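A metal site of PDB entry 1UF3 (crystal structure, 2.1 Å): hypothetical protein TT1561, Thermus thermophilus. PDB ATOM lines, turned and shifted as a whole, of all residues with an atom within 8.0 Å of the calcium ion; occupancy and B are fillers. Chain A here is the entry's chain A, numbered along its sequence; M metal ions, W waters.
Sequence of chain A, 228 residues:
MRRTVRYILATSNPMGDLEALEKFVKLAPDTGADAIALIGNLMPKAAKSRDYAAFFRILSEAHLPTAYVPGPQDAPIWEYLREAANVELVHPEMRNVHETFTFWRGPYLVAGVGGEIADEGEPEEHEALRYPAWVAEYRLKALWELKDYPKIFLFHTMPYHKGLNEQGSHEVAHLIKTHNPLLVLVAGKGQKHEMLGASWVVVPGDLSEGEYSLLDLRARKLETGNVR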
ATOM      1  N   MET A  43     -20.016   9.237 -25.928  1.00  0.00           N
ATOM      2  CA  MET A  43     -20.148  10.613 -25.411  1.00  0.00           C
ATOM      3  C   MET A  43     -21.228  10.692 -24.336  1.00  0.00           C
ATOM      4  O   MET A  43     -22.141   9.865 -24.303  1.00  0.00           O
ATOM      5  CB  MET A  43     -20.625  11.537 -26.546  1.00  0.00           C
ATOM      6  CG  MET A  43     -19.624  11.894 -27.594  1.00  0.00           C
ATOM      7  SD  MET A  43     -18.412  13.133 -26.848  1.00  0.00           S
ATOM      8  CE  MET A  43     -16.816  12.547 -27.795  1.00  0.00           C
ATOM      9  N   PRO A  44     -21.138  11.717 -23.454  1.00  0.00           N
ATOM     10  CA  PRO A  44     -22.149  11.890 -22.403  1.00  0.00           C
ATOM     11  C   PRO A  44     -23.365  12.441 -23.144  1.00  0.00           C
ATOM     12  O   PRO A  44     -23.226  13.005 -24.231  1.00  0.00           O
ATOM     13  CB  PRO A  44     -21.540  12.953 -21.499  1.00  0.00           C
ATOM     14  CG  PRO A  44     -20.070  12.866 -21.767  1.00  0.00           C
ATOM     15  CD  PRO A  44     -20.016  12.637 -23.259  1.00  0.00           C
ATOM     16  N   LYS A  45     -24.548  12.320 -22.559  1.00  0.00           N
ATOM     17  CA  LYS A  45     -25.769  12.835 -23.160  1.00  0.00           C
ATOM     18  C   LYS A  45     -25.602  14.294 -23.653  1.00  0.00           C
ATOM     19  O   LYS A  45     -26.055  14.641 -24.738  1.00  0.00           O
ATOM     20  CB  LYS A  45     -26.927  12.740 -22.156  1.00  0.00           C
ATOM     21  CG  LYS A  45     -28.231  13.397 -22.566  1.00  0.00           C
ATOM     22  CD  LYS A  45     -28.837  12.726 -23.782  1.00  0.00           C
ATOM     23  CE  LYS A  45     -30.109  13.417 -24.235  1.00  0.00           C
ATOM     24  NZ  LYS A  45     -31.165  13.384 -23.185  1.00  0.00           N
ATOM     25  N   ALA A  46     -24.935  15.116 -22.835  1.00  0.00           N
ATOM     26  CA  ALA A  46     -24.737  16.541 -23.143  1.00  0.00           C
ATOM     27  C   ALA A  46     -24.094  16.827 -24.501  1.00  0.00           C
ATOM     28  O   ALA A  46     -24.405  17.835 -25.132  1.00  0.00           O
ATOM     29  CB  ALA A  46     -23.893  17.208 -22.037  1.00  0.00           C
ATOM     30  N   ALA A  47     -23.188  15.958 -24.915  1.00  0.00           N
ATOM     31  CA  ALA A  47     -22.490  16.127 -26.185  1.00  0.00           C
ATOM     32  C   ALA A  47     -23.425  16.314 -27.384  1.00  0.00           C
ATOM     33  O   ALA A  47     -24.579  15.803 -27.405  1.00  0.00           O
ATOM     34  CB  ALA A  47     -21.569  14.928 -26.418  1.00  0.00           C
ATOM     35  N   LYS A  48     -22.911  17.060 -28.351  1.00  0.00           N
ATOM     36  CA  LYS A  48     -23.621  17.355 -29.607  1.00  0.00           C
ATOM     37  C   LYS A  48     -22.801  16.900 -30.818  1.00  0.00           C
ATOM     38  O   LYS A  48     -21.673  16.432 -30.682  1.00  0.00           O
ATOM     39  CB  LYS A  48     -23.884  18.861 -29.729  1.00  0.00           C
ATOM     40  CG  LYS A  48     -24.766  19.462 -28.628  1.00  0.00           C
ATOM     41  CD  LYS A  48     -25.156  20.917 -28.975  1.00  0.00           C
ATOM     42  CE  LYS A  48     -26.268  21.441 -28.070  1.00  0.00           C
ATOM     43  NZ  LYS A  48     -25.806  21.687 -26.669  1.00  0.00           N
ATOM     44  N   SER A  49     -23.359  17.069 -32.016  1.00  0.00           N
ATOM     45  CA  SER A  49     -22.680  16.663 -33.238  1.00  0.00           C
ATOM     46  C   SER A  49     -21.178  16.916 -33.302  1.00  0.00           C
ATOM     47  O   SER A  49     -20.397  15.978 -33.509  1.00  0.00           O
ATOM     48  CB  SER A  49     -23.351  17.314 -34.439  1.00  0.00           C
ATOM     49  OG  SER A  49     -24.690  16.877 -34.564  1.00  0.00           O
ATOM     50  N   ASP A  51     -18.995  17.193 -31.174  1.00  0.00           N
ATOM     51  CA  ASP A  51     -18.214  16.398 -30.231  1.00  0.00           C
ATOM     52  C   ASP A  51     -17.955  15.007 -30.829  1.00  0.00           C
ATOM     53  O   ASP A  51     -16.866  14.465 -30.737  1.00  0.00           O
ATOM     54  CB  ASP A  51     -18.972  16.266 -28.902  1.00  0.00           C
ATOM     55  CG  ASP A  51     -19.321  17.618 -28.287  1.00  0.00           C
ATOM     56  OD1 ASP A  51     -18.382  18.392 -28.046  1.00  0.00           O
ATOM     57  OD2 ASP A  51     -20.524  17.895 -28.037  1.00  0.00           O
ATOM     58  N   TYR A  52     -18.991  14.434 -31.432  1.00  0.00           N
ATOM     59  CA  TYR A  52     -18.845  13.120 -32.040  1.00  0.00           C
ATOM     60  C   TYR A  52     -17.831  13.218 -33.174  1.00  0.00           C
ATOM     61  O   TYR A  52     -17.021  12.315 -33.387  1.00  0.00           O
ATOM     62  CB  TYR A  52     -20.207  12.628 -32.549  1.00  0.00           C
ATOM     63  CG  TYR A  52     -21.092  12.107 -31.426  1.00  0.00           C
ATOM     64  CD1 TYR A  52     -22.107  12.893 -30.878  1.00  0.00           C
ATOM     65  CD2 TYR A  52     -20.885  10.831 -30.892  1.00  0.00           C
ATOM     66  CE1 TYR A  52     -22.888  12.416 -29.835  1.00  0.00           C
ATOM     67  CE2 TYR A  52     -21.669  10.347 -29.845  1.00  0.00           C
ATOM     68  CZ  TYR A  52     -22.671  11.145 -29.327  1.00  0.00           C
ATOM     69  OH  TYR A  52     -23.442  10.667 -28.282  1.00  0.00           O
ATOM     70  N   GLN A  73     -26.599   6.868 -23.367  1.00  0.00           N
ATOM     71  CA  GLN A  73     -26.498   8.327 -23.383  1.00  0.00           C
ATOM     72  C   GLN A  73     -26.147   9.008 -24.741  1.00  0.00           C
ATOM     73  O   GLN A  73     -26.107  10.243 -24.837  1.00  0.00           O
ATOM     74  CB  GLN A  73     -25.492   8.763 -22.319  1.00  0.00           C
ATOM     75  CG  GLN A  73     -26.012   8.610 -20.887  1.00  0.00           C
ATOM     76  CD  GLN A  73     -25.030   9.175 -19.872  1.00  0.00           C
ATOM     77  OE1 GLN A  73     -24.567  10.309 -20.010  1.00  0.00           O
ATOM     78  NE2 GLN A  73     -24.692   8.387 -18.850  1.00  0.00           N
ATOM     79  N   ASP A  74     -25.905   8.220 -25.785  1.00  0.00           N
ATOM     80  CA  ASP A  74     -25.549   8.762 -27.103  1.00  0.00           C
ATOM     81  C   ASP A  74     -26.795   9.212 -27.866  1.00  0.00           C
ATOM     82  O   ASP A  74     -27.054   8.758 -28.985  1.00  0.00           O
ATOM     83  CB  ASP A  74     -24.780   7.699 -27.919  1.00  0.00           C
ATOM     84  CG  ASP A  74     -23.370   7.493 -27.418  1.00  0.00           C
ATOM     85  OD1 ASP A  74     -22.584   8.470 -27.393  1.00  0.00           O
ATOM     86  OD2 ASP A  74     -23.030   6.345 -27.031  1.00  0.00           O
ATOM     87  N   ALA A  75     -27.565  10.109 -27.257  1.00  0.00           N
ATOM     88  CA  ALA A  75     -28.800  10.604 -27.861  1.00  0.00           C
ATOM     89  C   ALA A  75     -28.826  12.124 -28.082  1.00  0.00           C
ATOM     90  O   ALA A  75     -28.103  12.896 -27.428  1.00  0.00           O
ATOM     91  CB  ALA A  75     -29.989  10.154 -26.985  1.00  0.00           C
ATOM     92  N   PRO A  76     -29.630  12.586 -29.054  1.00  0.00           N
ATOM     93  CA  PRO A  76     -30.476  11.772 -29.938  1.00  0.00           C
ATOM     94  C   PRO A  76     -29.638  10.889 -30.880  1.00  0.00           C
ATOM     95  O   PRO A  76     -28.491  11.198 -31.208  1.00  0.00           O
ATOM     96  CB  PRO A  76     -31.303  12.826 -30.677  1.00  0.00           C
ATOM     97  CG  PRO A  76     -30.340  13.975 -30.781  1.00  0.00           C
ATOM     98  CD  PRO A  76     -29.746  14.009 -29.392  1.00  0.00           C
ATOM     99  N   ILE A  77     -30.235   9.783 -31.306  1.00  0.00           N
ATOM    100  CA  ILE A  77     -29.590   8.796 -32.161  1.00  0.00           C
ATOM    101  C   ILE A  77     -28.998   9.385 -33.450  1.00  0.00           C
ATOM    102  O   ILE A  77     -27.915   9.004 -33.885  1.00  0.00           O
ATOM    103  CB  ILE A  77     -30.611   7.661 -32.514  1.00  0.00           C
ATOM    104  CG1 ILE A  77     -29.959   6.567 -33.377  1.00  0.00           C
ATOM    105  CG2 ILE A  77     -31.779   8.256 -33.274  1.00  0.00           C
ATOM    106  CD1 ILE A  77     -28.907   5.754 -32.665  1.00  0.00           C
ATOM    107  N   GLU A  79     -27.558  12.209 -34.136  1.00  0.00           N
ATOM    108  CA  GLU A  79     -26.294  12.949 -34.076  1.00  0.00           C
ATOM    109  C   GLU A  79     -25.133  11.967 -34.162  1.00  0.00           C
ATOM    110  O   GLU A  79     -24.185  12.158 -34.951  1.00  0.00           O
ATOM    111  CB  GLU A  79     -26.187  13.780 -32.792  1.00  0.00           C
ATOM    112  CG  GLU A  79     -27.268  14.844 -32.681  1.00  0.00           C
ATOM    113  CD  GLU A  79     -26.919  16.001 -31.737  1.00  0.00           C
ATOM    114  OE1 GLU A  79     -27.642  17.003 -31.789  1.00  0.00           O
ATOM    115  OE2 GLU A  79     -25.933  15.918 -30.957  1.00  0.00           O
ATOM    116  N   TYR A  80     -25.190  10.926 -33.326  1.00  0.00           N
ATOM    117  CA  TYR A  80     -24.173   9.865 -33.355  1.00  0.00           C
ATOM    118  C   TYR A  80     -24.166   9.308 -34.783  1.00  0.00           C
ATOM    119  O   TYR A  80     -23.116   9.227 -35.421  1.00  0.00           O
ATOM    120  CB  TYR A  80     -24.556   8.747 -32.357  1.00  0.00           C
ATOM    121  CG  TYR A  80     -23.988   7.347 -32.664  1.00  0.00           C
ATOM    122  CD1 TYR A  80     -22.684   6.995 -32.287  1.00  0.00           C
ATOM    123  CD2 TYR A  80     -24.758   6.375 -33.310  1.00  0.00           C
ATOM    124  CE1 TYR A  80     -22.162   5.712 -32.538  1.00  0.00           C
ATOM    125  CE2 TYR A  80     -24.246   5.080 -33.568  1.00  0.00           C
ATOM    126  CZ  TYR A  80     -22.955   4.754 -33.176  1.00  0.00           C
ATOM    127  OH  TYR A  80     -22.440   3.482 -33.374  1.00  0.00           O
ATOM    128  N   HIS A 126     -34.431   9.778 -28.462  1.00  0.00           N
ATOM    129  CA  HIS A 126     -34.139  11.194 -28.320  1.00  0.00           C
ATOM    130  C   HIS A 126     -33.616  11.628 -26.939  1.00  0.00           C
ATOM    131  O   HIS A 126     -32.586  12.299 -26.865  1.00  0.00           O
ATOM    132  CB  HIS A 126     -35.363  12.004 -28.732  1.00  0.00           C
ATOM    133  CG  HIS A 126     -35.734  11.822 -30.170  1.00  0.00           C
ATOM    134  ND1 HIS A 126     -36.394  10.708 -30.631  1.00  0.00           N
ATOM    135  CD2 HIS A 126     -35.452  12.571 -31.265  1.00  0.00           C
ATOM    136  CE1 HIS A 126     -36.503  10.774 -31.939  1.00  0.00           C
ATOM    137  NE2 HIS A 126     -35.945  11.893 -32.357  1.00  0.00           N
ATOM    138  N   GLU A 127     -34.312  11.242 -25.877  1.00  0.00           N
ATOM    139  CA  GLU A 127     -33.871  11.579 -24.523  1.00  0.00           C
ATOM    140  C   GLU A 127     -32.794  10.577 -24.097  1.00  0.00           C
ATOM    141  O   GLU A 127     -31.973  10.836 -23.219  1.00  0.00           O
ATOM    142  CB  GLU A 127     -35.055  11.515 -23.548  1.00  0.00           C
ATOM    143  CG  GLU A 127     -36.272  12.321 -23.981  1.00  0.00           C
ATOM    144  CD  GLU A 127     -37.520  11.933 -23.205  1.00  0.00           C
ATOM    145  OE1 GLU A 127     -37.787  10.712 -23.077  1.00  0.00           O
ATOM    146  OE2 GLU A 127     -38.250  12.832 -22.727  1.00  0.00           O
HETATM  147 CA    CA M   1     -26.359  14.419 -27.117  1.00  0.00          CA
HETATM  148  O   HOH W   1     -27.223  16.312 -28.456  1.00  0.00           O
HETATM  149  O   HOH W   2     -24.648  12.689 -26.598  1.00  0.00           O
HETATM  150  O   HOH W   3     -28.209  16.299 -26.186  1.00  0.00           O
HETATM  151  O   HOH W   4     -25.800  13.716 -29.496  1.00  0.00           O
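Within 4 Å of the calcium ion: Lys 45, Ala 47 and Ala 75.
Water W2 lies within hydrogen-bond range of the backbone carbonyl oxygen (O) of Pro 44 (2.8 Å), the side-chain hydroxyl (OH) of Tyr 52 (2.9 Å) and the backbone carbonyl oxygen (O) of Gln 73 (3.3 Å).
The calcium ion is bound by O of Ala 47, 2.3 Å away.
O of Ala 75 binds the calcium ion, 2.3 Å away.
O of Lys 45 is bound to the calcium ion (2.4 Å).
Water W1 binds the calcium ion, at 2.5 Å.
Water W2 is bound to the calcium ion (2.5 Å).
The calcium ion is bound by water W4 (2.5 Å).
The calcium ion is bound by water W3.
N of Lys 45 lies within hydrogen-bond range of OE1 of Gln 73 (3.2 Å).
The side-chain amino group (NZ) of Lys 45 lies within hydrogen-bond range of the backbone carbonyl oxygen (O) of Glu 127 (2.7 Å).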
